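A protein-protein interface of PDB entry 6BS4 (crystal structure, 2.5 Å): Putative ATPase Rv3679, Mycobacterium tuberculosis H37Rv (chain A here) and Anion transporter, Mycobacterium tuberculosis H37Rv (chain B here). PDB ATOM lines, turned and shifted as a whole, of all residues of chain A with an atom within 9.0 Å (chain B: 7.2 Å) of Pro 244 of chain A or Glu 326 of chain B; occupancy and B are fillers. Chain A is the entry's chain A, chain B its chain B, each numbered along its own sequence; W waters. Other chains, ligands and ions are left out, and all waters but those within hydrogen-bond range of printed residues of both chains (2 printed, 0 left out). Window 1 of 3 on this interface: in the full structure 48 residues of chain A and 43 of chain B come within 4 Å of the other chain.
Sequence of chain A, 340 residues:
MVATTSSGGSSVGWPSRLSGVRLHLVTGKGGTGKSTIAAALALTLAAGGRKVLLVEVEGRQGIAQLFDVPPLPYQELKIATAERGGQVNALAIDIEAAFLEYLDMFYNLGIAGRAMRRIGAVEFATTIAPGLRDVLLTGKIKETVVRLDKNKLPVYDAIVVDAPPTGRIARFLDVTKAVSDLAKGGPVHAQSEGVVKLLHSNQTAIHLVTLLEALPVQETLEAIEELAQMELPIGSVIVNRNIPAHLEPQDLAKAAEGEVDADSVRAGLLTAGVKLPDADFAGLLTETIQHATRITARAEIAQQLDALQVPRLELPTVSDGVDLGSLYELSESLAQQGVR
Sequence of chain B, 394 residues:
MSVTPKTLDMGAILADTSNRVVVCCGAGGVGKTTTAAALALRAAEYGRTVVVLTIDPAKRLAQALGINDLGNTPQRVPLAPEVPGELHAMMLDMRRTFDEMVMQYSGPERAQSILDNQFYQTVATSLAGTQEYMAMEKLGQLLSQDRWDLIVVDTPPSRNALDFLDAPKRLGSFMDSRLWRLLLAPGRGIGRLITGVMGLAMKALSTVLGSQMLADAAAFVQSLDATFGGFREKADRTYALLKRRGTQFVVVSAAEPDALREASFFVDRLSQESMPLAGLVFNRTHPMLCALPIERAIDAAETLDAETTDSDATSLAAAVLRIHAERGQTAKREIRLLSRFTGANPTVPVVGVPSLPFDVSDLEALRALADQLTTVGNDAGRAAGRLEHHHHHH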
ATOM      1  N   ARG A 241      16.956 -17.182   4.756  1.00  0.00           N
ATOM      2  CA  ARG A 241      16.137 -15.995   4.501  1.00  0.00           C
ATOM      3  C   ARG A 241      16.703 -15.097   3.410  1.00  0.00           C
ATOM      4  O   ARG A 241      16.927 -13.893   3.600  1.00  0.00           O
ATOM      5  CB  ARG A 241      15.843 -15.208   5.787  1.00  0.00           C
ATOM      6  CG  ARG A 241      15.312 -16.088   6.898  1.00  0.00           C
ATOM      7  CD  ARG A 241      14.543 -15.354   7.955  1.00  0.00           C
ATOM      8  NE  ARG A 241      15.250 -14.185   8.455  1.00  0.00           N
ATOM      9  CZ  ARG A 241      14.804 -13.406   9.429  1.00  0.00           C
ATOM     10  NH1 ARG A 241      13.661 -13.689  10.044  1.00  0.00           N
ATOM     11  NH2 ARG A 241      15.499 -12.341   9.804  1.00  0.00           N
ATOM     12  N   ASN A 242      16.891 -15.700   2.241  1.00  0.00           N
ATOM     13  CA  ASN A 242      17.323 -14.970   1.085  1.00  0.00           C
ATOM     14  C   ASN A 242      16.148 -14.153   0.570  1.00  0.00           C
ATOM     15  O   ASN A 242      14.987 -14.493   0.833  1.00  0.00           O
ATOM     16  CB  ASN A 242      17.842 -15.905   0.036  1.00  0.00           C
ATOM     17  CG  ASN A 242      19.216 -16.383   0.349  1.00  0.00           C
ATOM     18  OD1 ASN A 242      20.188 -15.624   0.295  1.00  0.00           O
ATOM     19  ND2 ASN A 242      19.315 -17.651   0.691  1.00  0.00           N
ATOM     20  N   ILE A 243      16.459 -13.023  -0.087  1.00  0.00           N
ATOM     21  CA  ILE A 243      15.454 -12.123  -0.636  1.00  0.00           C
ATOM     22  C   ILE A 243      15.754 -11.878  -2.113  1.00  0.00           C
ATOM     23  O   ILE A 243      16.919 -12.015  -2.513  1.00  0.00           O
ATOM     24  CB  ILE A 243      15.291 -10.815   0.205  1.00  0.00           C
ATOM     25  CG1 ILE A 243      16.580  -9.948   0.196  1.00  0.00           C
ATOM     26  CG2 ILE A 243      14.800 -11.144   1.627  1.00  0.00           C
ATOM     27  CD1 ILE A 243      16.430  -8.571   0.702  1.00  0.00           C
ATOM     28  N   PRO A 244      14.735 -11.548  -2.954  1.00  0.00           N
ATOM     29  CA  PRO A 244      15.032 -11.302  -4.380  1.00  0.00           C
ATOM     30  C   PRO A 244      15.724  -9.968  -4.606  1.00  0.00           C
ATOM     31  O   PRO A 244      15.440  -8.993  -3.902  1.00  0.00           O
ATOM     32  CB  PRO A 244      13.658 -11.337  -5.049  1.00  0.00           C
ATOM     33  CG  PRO A 244      12.702 -11.003  -3.981  1.00  0.00           C
ATOM     34  CD  PRO A 244      13.301 -11.346  -2.652  1.00  0.00           C
ATOM     35  N   ALA A 245      16.742  -9.987  -5.462  1.00  0.00           N
ATOM     36  CA  ALA A 245      17.417  -8.738  -5.857  1.00  0.00           C
ATOM     37  C   ALA A 245      16.471  -7.938  -6.746  1.00  0.00           C
ATOM     38  O   ALA A 245      16.448  -6.728  -6.624  1.00  0.00           O
ATOM     39  CB  ALA A 245      18.713  -9.039  -6.546  1.00  0.00           C
ATOM     40  N   HIS A 246      15.707  -8.637  -7.586  1.00  0.00           N
ATOM     41  CA  HIS A 246      14.741  -8.039  -8.513  1.00  0.00           C
ATOM     42  C   HIS A 246      15.357  -7.004  -9.452  1.00  0.00           C
ATOM     43  O   HIS A 246      14.643  -6.305 -10.170  1.00  0.00           O
ATOM     44  CB  HIS A 246      13.534  -7.452  -7.767  1.00  0.00           C
ATOM     45  CG  HIS A 246      12.525  -8.476  -7.350  1.00  0.00           C
ATOM     46  ND1 HIS A 246      12.324  -9.650  -8.043  1.00  0.00           N
ATOM     47  CD2 HIS A 246      11.658  -8.502  -6.309  1.00  0.00           C
ATOM     48  CE1 HIS A 246      11.379 -10.355  -7.447  1.00  0.00           C
ATOM     49  NE2 HIS A 246      10.958  -9.680  -6.393  1.00  0.00           N
ATOM     50  N   LEU A 247      16.683  -6.910  -9.441  1.00  0.00           N
ATOM     51  CA  LEU A 247      17.384  -5.966 -10.305  1.00  0.00           C
ATOM     52  C   LEU A 247      18.590  -6.610 -10.982  1.00  0.00           C
ATOM     53  O   LEU A 247      19.226  -7.501 -10.418  1.00  0.00           O
ATOM     54  CB  LEU A 247      17.825  -4.737  -9.507  1.00  0.00           C
ATOM     55  CG  LEU A 247      16.952  -3.488  -9.652  1.00  0.00           C
ATOM     56  CD1 LEU A 247      17.329  -2.446  -8.609  1.00  0.00           C
ATOM     57  CD2 LEU A 247      17.061  -2.914 -11.055  1.00  0.00           C
ATOM     58  N   LEU A 252      21.492  -2.551 -10.514  1.00  0.00           N
ATOM     59  CA  LEU A 252      21.605  -2.668  -9.057  1.00  0.00           C
ATOM     60  C   LEU A 252      22.802  -1.892  -8.536  1.00  0.00           C
ATOM     61  O   LEU A 252      22.651  -1.117  -7.590  1.00  0.00           O
ATOM     62  CB  LEU A 252      21.705  -4.149  -8.649  1.00  0.00           C
ATOM     63  CG  LEU A 252      21.673  -4.440  -7.153  1.00  0.00           C
ATOM     64  CD1 LEU A 252      20.252  -4.664  -6.672  1.00  0.00           C
ATOM     65  CD2 LEU A 252      22.531  -5.623  -6.831  1.00  0.00           C
ATOM     66  N   GLU A 287      12.955   4.266  -3.231  1.00  0.00           N
ATOM     67  CA  GLU A 287      12.559   2.935  -2.763  1.00  0.00           C
ATOM     68  C   GLU A 287      13.457   1.883  -3.407  1.00  0.00           C
ATOM     69  O   GLU A 287      13.814   0.905  -2.747  1.00  0.00           O
ATOM     70  CB  GLU A 287      11.091   2.632  -3.125  1.00  0.00           C
ATOM     71  CG  GLU A 287      10.075   3.166  -2.132  1.00  0.00           C
ATOM     72  CD  GLU A 287       8.612   2.893  -2.436  1.00  0.00           C
ATOM     73  OE1 GLU A 287       8.322   2.048  -3.312  1.00  0.00           O
ATOM     74  OE2 GLU A 287       7.748   3.524  -1.786  1.00  0.00           O
ATOM     75  N   HIS A 291      16.497  -0.407  -1.773  1.00  0.00           N
ATOM     76  CA  HIS A 291      16.520  -1.850  -2.009  1.00  0.00           C
ATOM     77  C   HIS A 291      17.906  -2.264  -2.518  1.00  0.00           C
ATOM     78  O   HIS A 291      18.499  -3.203  -1.984  1.00  0.00           O
ATOM     79  CB  HIS A 291      15.426  -2.246  -3.015  1.00  0.00           C
ATOM     80  CG  HIS A 291      15.483  -3.686  -3.436  1.00  0.00           C
ATOM     81  ND1 HIS A 291      14.914  -4.687  -2.670  1.00  0.00           N
ATOM     82  CD2 HIS A 291      16.083  -4.249  -4.508  1.00  0.00           C
ATOM     83  CE1 HIS A 291      15.166  -5.814  -3.306  1.00  0.00           C
ATOM     84  NE2 HIS A 291      15.863  -5.601  -4.418  1.00  0.00           N
ATOM     85  N   ALA A 292      18.416  -1.551  -3.542  1.00  0.00           N
ATOM     86  CA  ALA A 292      19.731  -1.770  -4.158  1.00  0.00           C
ATOM     87  C   ALA A 292      20.862  -1.687  -3.136  1.00  0.00           C
ATOM     88  O   ALA A 292      21.761  -2.525  -3.173  1.00  0.00           O
ATOM     89  CB  ALA A 292      19.960  -0.767  -5.271  1.00  0.00           C
ATOM     90  N   ARG A 294      20.545  -2.278   0.120  1.00  0.00           N
ATOM     91  CA  ARG A 294      20.427  -3.445   0.994  1.00  0.00           C
ATOM     92  C   ARG A 294      21.030  -4.704   0.358  1.00  0.00           C
ATOM     93  O   ARG A 294      21.745  -5.430   1.043  1.00  0.00           O
ATOM     94  CB  ARG A 294      18.966  -3.694   1.412  1.00  0.00           C
ATOM     95  CG  ARG A 294      18.836  -4.787   2.465  1.00  0.00           C
ATOM     96  CD  ARG A 294      17.401  -5.076   2.802  1.00  0.00           C
ATOM     97  NE  ARG A 294      17.288  -6.340   3.523  1.00  0.00           N
ATOM     98  CZ  ARG A 294      16.144  -6.854   3.950  1.00  0.00           C
ATOM     99  NH1 ARG A 294      15.001  -6.214   3.741  1.00  0.00           N
ATOM    100  NH2 ARG A 294      16.130  -8.013   4.594  1.00  0.00           N
ATOM    101  N   ILE A 295      20.729  -4.964  -0.933  1.00  0.00           N
ATOM    102  CA  ILE A 295      21.239  -6.118  -1.683  1.00  0.00           C
ATOM    103  C   ILE A 295      22.768  -6.035  -1.785  1.00  0.00           C
ATOM    104  O   ILE A 295      23.442  -7.025  -1.513  1.00  0.00           O
ATOM    105  CB  ILE A 295      20.546  -6.264  -3.087  1.00  0.00           C
ATOM    106  CG1 ILE A 295      18.990  -6.269  -3.003  1.00  0.00           C
ATOM    107  CG2 ILE A 295      21.056  -7.484  -3.873  1.00  0.00           C
ATOM    108  CD1 ILE A 295      18.325  -7.419  -2.165  1.00  0.00           C
ATOM    109  N   ARG A 298      24.391  -6.758   1.509  1.00  0.00           N
ATOM    110  CA  ARG A 298      24.234  -8.202   1.733  1.00  0.00           C
ATOM    111  C   ARG A 298      25.203  -9.030   0.890  1.00  0.00           C
ATOM    112  O   ARG A 298      25.684 -10.054   1.368  1.00  0.00           O
ATOM    113  CB  ARG A 298      22.798  -8.657   1.481  1.00  0.00           C
ATOM    114  CG  ARG A 298      21.868  -8.352   2.643  1.00  0.00           C
ATOM    115  CD  ARG A 298      20.405  -8.394   2.223  1.00  0.00           C
ATOM    116  NE  ARG A 298      19.970  -9.744   1.859  1.00  0.00           N
ATOM    117  CZ  ARG A 298      19.601 -10.676   2.732  1.00  0.00           C
ATOM    118  NH1 ARG A 298      19.619 -10.418   4.031  1.00  0.00           N
ATOM    119  NH2 ARG A 298      19.226 -11.877   2.314  1.00  0.00           N
ATOM    120  N   LEU A 315      18.325 -20.940   1.285  1.00  0.00           N
ATOM    121  CA  LEU A 315      16.909 -21.062   1.598  1.00  0.00           C
ATOM    122  C   LEU A 315      16.198 -19.709   1.444  1.00  0.00           C
ATOM    123  O   LEU A 315      16.790 -18.664   1.744  1.00  0.00           O
ATOM    124  CB  LEU A 315      16.690 -21.676   2.993  1.00  0.00           C
ATOM    125  CG  LEU A 315      17.121 -23.141   3.135  1.00  0.00           C
ATOM    126  CD1 LEU A 315      16.974 -23.597   4.558  1.00  0.00           C
ATOM    127  CD2 LEU A 315      16.289 -24.070   2.210  1.00  0.00           C
ATOM    128  N   PRO A 316      14.960 -19.690   0.908  1.00  0.00           N
ATOM    129  CA  PRO A 316      14.260 -18.404   0.755  1.00  0.00           C
ATOM    130  C   PRO A 316      13.648 -17.933   2.077  1.00  0.00           C
ATOM    131  O   PRO A 316      13.701 -18.648   3.082  1.00  0.00           O
ATOM    132  CB  PRO A 316      13.148 -18.745  -0.252  1.00  0.00           C
ATOM    133  CG  PRO A 316      12.801 -20.169   0.070  1.00  0.00           C
ATOM    134  CD  PRO A 316      14.117 -20.823   0.456  1.00  0.00           C
ATOM    135  N   THR A 317      13.030 -16.740   2.055  1.00  0.00           N
ATOM    136  CA  THR A 317      12.297 -16.207   3.186  1.00  0.00           C
ATOM    137  C   THR A 317      10.855 -16.684   3.053  1.00  0.00           C
ATOM    138  O   THR A 317      10.254 -16.547   1.983  1.00  0.00           O
ATOM    139  CB  THR A 317      12.311 -14.666   3.184  1.00  0.00           C
ATOM    140  OG1 THR A 317      13.656 -14.206   3.194  1.00  0.00           O
ATOM    141  CG2 THR A 317      11.548 -14.065   4.373  1.00  0.00           C
ATOM    142  N   HIS B 286       9.243   0.011   7.102  1.00  0.00           N
ATOM    143  CA  HIS B 286       9.389   0.321   5.686  1.00  0.00           C
ATOM    144  C   HIS B 286       8.249   1.224   5.223  1.00  0.00           C
ATOM    145  O   HIS B 286       7.314   0.744   4.569  1.00  0.00           O
ATOM    146  CB  HIS B 286       9.540  -0.969   4.859  1.00  0.00           C
ATOM    147  CG  HIS B 286      10.762  -1.743   5.235  1.00  0.00           C
ATOM    148  ND1 HIS B 286      10.781  -2.549   6.358  1.00  0.00           N
ATOM    149  CD2 HIS B 286      11.991  -1.745   4.674  1.00  0.00           C
ATOM    150  CE1 HIS B 286      12.009  -3.043   6.429  1.00  0.00           C
ATOM    151  NE2 HIS B 286      12.777  -2.582   5.444  1.00  0.00           N
ATOM    152  N   MET B 288       5.876   3.740   3.139  1.00  0.00           N
ATOM    153  CA  MET B 288       5.694   3.884   1.703  1.00  0.00           C
ATOM    154  C   MET B 288       6.064   5.280   1.238  1.00  0.00           C
ATOM    155  O   MET B 288       5.657   6.272   1.851  1.00  0.00           O
ATOM    156  CB  MET B 288       4.296   3.448   1.264  1.00  0.00           C
ATOM    157  CG  MET B 288       4.066   1.943   1.394  1.00  0.00           C
ATOM    158  SD  MET B 288       5.454   0.887   0.862  1.00  0.00           S
ATOM    159  CE  MET B 288       5.393   1.097  -0.914  1.00  0.00           C
ATOM    160  N   ILE B 294      -0.585  -1.696  -4.469  1.00  0.00           N
ATOM    161  CA  ILE B 294       0.098  -2.975  -4.696  1.00  0.00           C
ATOM    162  C   ILE B 294      -0.504  -3.710  -5.890  1.00  0.00           C
ATOM    163  O   ILE B 294       0.242  -4.088  -6.797  1.00  0.00           O
ATOM    164  CB  ILE B 294       0.175  -3.855  -3.402  1.00  0.00           C
ATOM    165  CG1 ILE B 294       0.831  -3.111  -2.212  1.00  0.00           C
ATOM    166  CG2 ILE B 294       0.848  -5.216  -3.649  1.00  0.00           C
ATOM    167  CD1 ILE B 294       2.128  -2.328  -2.524  1.00  0.00           C
ATOM    168  N   ALA B 297       0.518  -1.961  -9.067  1.00  0.00           N
ATOM    169  CA  ALA B 297       1.954  -2.169  -9.292  1.00  0.00           C
ATOM    170  C   ALA B 297       2.261  -3.564  -9.825  1.00  0.00           C
ATOM    171  O   ALA B 297       3.097  -3.699 -10.723  1.00  0.00           O
ATOM    172  CB  ALA B 297       2.731  -1.918  -8.006  1.00  0.00           C
ATOM    173  N   ILE B 298       1.581  -4.593  -9.273  1.00  0.00           N
ATOM    174  CA  ILE B 298       1.721  -5.993  -9.670  1.00  0.00           C
ATOM    175  C   ILE B 298       1.274  -6.159 -11.125  1.00  0.00           C
ATOM    176  O   ILE B 298       2.024  -6.730 -11.919  1.00  0.00           O
ATOM    177  CB  ILE B 298       0.994  -6.937  -8.659  1.00  0.00           C
ATOM    178  CG1 ILE B 298       1.814  -7.120  -7.348  1.00  0.00           C
ATOM    179  CG2 ILE B 298       0.576  -8.291  -9.272  1.00  0.00           C
ATOM    180  CD1 ILE B 298       3.203  -7.876  -7.453  1.00  0.00           C
ATOM    181  N   LEU B 321       8.838  -1.651 -10.192  1.00  0.00           N
ATOM    182  CA  LEU B 321       7.455  -1.857  -9.780  1.00  0.00           C
ATOM    183  C   LEU B 321       7.345  -3.051  -8.841  1.00  0.00           C
ATOM    184  O   LEU B 321       6.505  -3.031  -7.938  1.00  0.00           O
ATOM    185  CB  LEU B 321       6.555  -2.028 -11.025  1.00  0.00           C
ATOM    186  CG  LEU B 321       6.393  -0.831 -11.990  1.00  0.00           C
ATOM    187  CD1 LEU B 321       5.597  -1.178 -13.251  1.00  0.00           C
ATOM    188  CD2 LEU B 321       5.757   0.344 -11.283  1.00  0.00           C
ATOM    189  N   ARG B 322       8.204  -4.078  -9.042  1.00  0.00           N
ATOM    190  CA  ARG B 322       8.265  -5.273  -8.201  1.00  0.00           C
ATOM    191  C   ARG B 322       8.860  -4.935  -6.829  1.00  0.00           C
ATOM    192  O   ARG B 322       8.394  -5.484  -5.832  1.00  0.00           O
ATOM    193  CB  ARG B 322       9.069  -6.397  -8.872  1.00  0.00           C
ATOM    194  CG  ARG B 322       8.371  -7.047 -10.055  1.00  0.00           C
ATOM    195  CD  ARG B 322       8.383  -8.560  -9.961  1.00  0.00           C
ATOM    196  NE  ARG B 322       7.921  -9.176 -11.207  1.00  0.00           N
ATOM    197  CZ  ARG B 322       6.650  -9.451 -11.490  1.00  0.00           C
ATOM    198  NH1 ARG B 322       5.690  -9.167 -10.617  1.00  0.00           N
ATOM    199  NH2 ARG B 322       6.329 -10.010 -12.648  1.00  0.00           N
ATOM    200  N   ILE B 323       9.872  -4.030  -6.777  1.00  0.00           N
ATOM    201  CA  ILE B 323      10.514  -3.548  -5.541  1.00  0.00           C
ATOM    202  C   ILE B 323       9.432  -2.906  -4.670  1.00  0.00           C
ATOM    203  O   ILE B 323       9.282  -3.257  -3.500  1.00  0.00           O
ATOM    204  CB  ILE B 323      11.624  -2.478  -5.825  1.00  0.00           C
ATOM    205  CG1 ILE B 323      12.728  -2.946  -6.824  1.00  0.00           C
ATOM    206  CG2 ILE B 323      12.246  -1.938  -4.536  1.00  0.00           C
ATOM    207  CD1 ILE B 323      13.499  -4.145  -6.541  1.00  0.00           C
ATOM    208  N   HIS B 324       8.703  -1.944  -5.262  1.00  0.00           N
ATOM    209  CA  HIS B 324       7.633  -1.159  -4.661  1.00  0.00           C
ATOM    210  C   HIS B 324       6.521  -2.037  -4.082  1.00  0.00           C
ATOM    211  O   HIS B 324       6.111  -1.820  -2.940  1.00  0.00           O
ATOM    212  CB  HIS B 324       7.095  -0.162  -5.701  1.00  0.00           C
ATOM    213  CG  HIS B 324       5.823   0.509  -5.307  1.00  0.00           C
ATOM    214  ND1 HIS B 324       5.817   1.590  -4.453  1.00  0.00           N
ATOM    215  CD2 HIS B 324       4.551   0.211  -5.651  1.00  0.00           C
ATOM    216  CE1 HIS B 324       4.544   1.919  -4.308  1.00  0.00           C
ATOM    217  NE2 HIS B 324       3.748   1.115  -5.009  1.00  0.00           N
ATOM    218  N   ALA B 325       6.050  -3.023  -4.868  1.00  0.00           N
ATOM    219  CA  ALA B 325       4.993  -3.968  -4.495  1.00  0.00           C
ATOM    220  C   ALA B 325       5.408  -4.835  -3.303  1.00  0.00           C
ATOM    221  O   ALA B 325       4.582  -5.131  -2.436  1.00  0.00           O
ATOM    222  CB  ALA B 325       4.640  -4.848  -5.685  1.00  0.00           C
ATOM    223  N   GLU B 326       6.692  -5.245  -3.279  1.00  0.00           N
ATOM    224  CA  GLU B 326       7.314  -6.059  -2.238  1.00  0.00           C
ATOM    225  C   GLU B 326       7.429  -5.216  -0.963  1.00  0.00           C
ATOM    226  O   GLU B 326       7.119  -5.714   0.121  1.00  0.00           O
ATOM    227  CB  GLU B 326       8.667  -6.584  -2.750  1.00  0.00           C
ATOM    228  CG  GLU B 326       9.726  -6.940  -1.721  1.00  0.00           C
ATOM    229  CD  GLU B 326      10.896  -7.680  -2.336  1.00  0.00           C
ATOM    230  OE1 GLU B 326      11.969  -7.060  -2.522  1.00  0.00           O
ATOM    231  OE2 GLU B 326      10.731  -8.881  -2.649  1.00  0.00           O
ATOM    232  N   ARG B 327       7.823  -3.934  -1.101  1.00  0.00           N
ATOM    233  CA  ARG B 327       7.900  -2.998   0.017  1.00  0.00           C
ATOM    234  C   ARG B 327       6.498  -2.733   0.604  1.00  0.00           C
ATOM    235  O   ARG B 327       6.353  -2.718   1.824  1.00  0.00           O
ATOM    236  CB  ARG B 327       8.600  -1.686  -0.380  1.00  0.00           C
ATOM    237  CG  ARG B 327       8.785  -0.752   0.804  1.00  0.00           C
ATOM    238  CD  ARG B 327       9.116   0.651   0.383  1.00  0.00           C
ATOM    239  NE  ARG B 327      10.551   0.885   0.478  1.00  0.00           N
ATOM    240  CZ  ARG B 327      11.135   1.606   1.428  1.00  0.00           C
ATOM    241  NH1 ARG B 327      10.408   2.197   2.361  1.00  0.00           N
ATOM    242  NH2 ARG B 327      12.450   1.752   1.442  1.00  0.00           N
ATOM    243  N   GLY B 328       5.497  -2.557  -0.258  1.00  0.00           N
ATOM    244  CA  GLY B 328       4.117  -2.322   0.153  1.00  0.00           C
ATOM    245  C   GLY B 328       3.507  -3.472   0.927  1.00  0.00           C
ATOM    246  O   GLY B 328       2.755  -3.244   1.880  1.00  0.00           O
ATOM    247  N   GLN B 329       3.844  -4.722   0.530  1.00  0.00           N
ATOM    248  CA  GLN B 329       3.407  -5.954   1.191  1.00  0.00           C
ATOM    249  C   GLN B 329       4.038  -6.046   2.562  1.00  0.00           C
ATOM    250  O   GLN B 329       3.379  -6.476   3.511  1.00  0.00           O
ATOM    251  CB  GLN B 329       3.788  -7.180   0.357  1.00  0.00           C
ATOM    252  CG  GLN B 329       2.829  -7.446  -0.792  1.00  0.00           C
ATOM    253  CD  GLN B 329       3.357  -8.546  -1.667  1.00  0.00           C
ATOM    254  OE1 GLN B 329       4.151  -8.312  -2.583  1.00  0.00           O
ATOM    255  NE2 GLN B 329       2.933  -9.771  -1.397  1.00  0.00           N
ATOM    256  N   THR B 330       5.317  -5.605   2.663  1.00  0.00           N
ATOM    257  CA  THR B 330       6.113  -5.547   3.886  1.00  0.00           C
ATOM    258  C   THR B 330       5.510  -4.504   4.815  1.00  0.00           C
ATOM    259  O   THR B 330       5.359  -4.778   6.005  1.00  0.00           O
ATOM    260  CB  THR B 330       7.596  -5.285   3.562  1.00  0.00           C
ATOM    261  OG1 THR B 330       8.137  -6.420   2.884  1.00  0.00           O
ATOM    262  CG2 THR B 330       8.419  -4.976   4.793  1.00  0.00           C
ATOM    263  N   ALA B 331       5.148  -3.324   4.268  1.00  0.00           N
ATOM    264  CA  ALA B 331       4.514  -2.239   5.011  1.00  0.00           C
ATOM    265  C   ALA B 331       3.164  -2.711   5.565  1.00  0.00           C
ATOM    266  O   ALA B 331       2.898  -2.508   6.743  1.00  0.00           O
ATOM    267  CB  ALA B 331       4.335  -1.028   4.114  1.00  0.00           C
ATOM    268  N   LYS B 332       2.374  -3.433   4.748  1.00  0.00           N
ATOM    269  CA  LYS B 332       1.076  -4.018   5.103  1.00  0.00           C
ATOM    270  C   LYS B 332       1.164  -4.959   6.305  1.00  0.00           C
ATOM    271  O   LYS B 332       0.324  -4.850   7.199  1.00  0.00           O
ATOM    272  CB  LYS B 332       0.455  -4.746   3.899  1.00  0.00           C
ATOM    273  CG  LYS B 332      -0.946  -4.254   3.511  1.00  0.00           C
ATOM    274  CD  LYS B 332      -0.918  -3.028   2.573  1.00  0.00           C
ATOM    275  CE  LYS B 332      -2.305  -2.645   2.103  1.00  0.00           C
ATOM    276  NZ  LYS B 332      -2.302  -1.383   1.316  1.00  0.00           N
ATOM    277  N   ARG B 333       2.182  -5.858   6.341  1.00  0.00           N
ATOM    278  CA  ARG B 333       2.409  -6.784   7.462  1.00  0.00           C
ATOM    279  C   ARG B 333       2.798  -6.012   8.735  1.00  0.00           C
ATOM    280  O   ARG B 333       2.332  -6.367   9.820  1.00  0.00           O
ATOM    281  CB  ARG B 333       3.489  -7.832   7.130  1.00  0.00           C
ATOM    282  CG  ARG B 333       3.103  -8.772   5.983  1.00  0.00           C
ATOM    283  CD  ARG B 333       4.140  -9.843   5.682  1.00  0.00           C
ATOM    284  NE  ARG B 333       5.318  -9.309   4.995  1.00  0.00           N
ATOM    285  CZ  ARG B 333       6.473  -9.037   5.596  1.00  0.00           C
ATOM    286  NH1 ARG B 333       6.617  -9.251   6.897  1.00  0.00           N
ATOM    287  NH2 ARG B 333       7.491  -8.555   4.901  1.00  0.00           N
HETATM  288  O   HOH W   1       8.710  -9.415  -4.381  1.00  0.00           O
HETATM  289  O   HOH W   2      14.582  -3.400   2.566  1.00  0.00           O
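Water W1 lies within hydrogen-bond range of OE2 of Glu 326 of chain B (2.7 Å) and NE2 of His 246 of chain A (3.0 Å).
Water W2 lies within hydrogen-bond range of NH1 of Arg 294 of chain A and NE2 of His 286 of chain B.
O of Pro 244 of chain A lies close to NE2 of His 291 of chain A, 3.5 Å away.
The side-chain sulfur (SD) of Met 288 of chain B lies close to the backbone NH (N) of Gly 328 of chain B (3.6 Å).
The backbone carbonyl oxygen (O) of Ala 245 of chain A lies within hydrogen-bond range of a ring nitrogen (NE2) of His 291 of chain A (2.5 Å).
O of Glu 326 of chain B is in hydrogen-bond range of OG1 of Thr 330 of chain B (3.0 Å).
OE2 of Glu 326 of chain B touches CG of Pro 244 of chain A (3.2 Å).
O of Ala 245 of chain A touches CD1 of Ile 323 of chain B (3.9 Å).
Ile 323 of chain B touches His 246 of chain A.
Glu 326 of chain B touches His 246 of chain A.
Met 288 of chain B touches Glu 287 of chain A.
Glu 287 of chain A touches Ile 323 of chain B (O to CG2, 3.7 Å).
Glu 287 of chain A touches Arg 327 of chain B.
Ile 323 of chain B touches His 291 of chain A (CD1 to CD2, 3.3 Å).
His 291 of chain A touches Glu 326 of chain B (CE1 to OE1, 3.5 Å).
Arg 241 of chain A touches none of the printed residues of chain B.
Printed residues of chain B within 4 Å of His 246 of chain A: Ile 323 and Glu 326.
Ala 297 of chain B touches none of the printed residues of chain A.
Of the printed residues of chain A, His 324 of chain B touches Glu 287 (2.8 Å).
No residue of chain A comes within 4 Å of Ala 325 of chain B.
Of chain A, only Pro 244 (3.2 Å), His 246 (3.8 Å) and His 291 (3.5 Å) come within 4 Å of Glu 326 of chain B.
Of the printed residues of chain A, Arg 327 of chain B touches Glu 287 (3.5 Å).
The nearest residue of chain A that does not touch Glu 326 of chain B is Ile 243 of chain A (5.7 Å).
OE1 of Glu 287 of chain A is in hydrogen-bond range of ND1 of His 324 of chain B (2.8 Å).
Hydrophobic or aromatic side chains of chain B within 4 Å of the printed part of chain A: Met 288, Ile 323 and His 324.
Of the 17 printed residues of chain A, 5 touch a printed residue of chain B.
Hydrophobic or aromatic side chains of chain A that line the printed part of chain B: Pro 244, His 246 and His 291.
Among the printed residues, no Asp or Glu carboxylate lies within 4 Å of a Lys or Arg side-chain nitrogen of the other chain.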
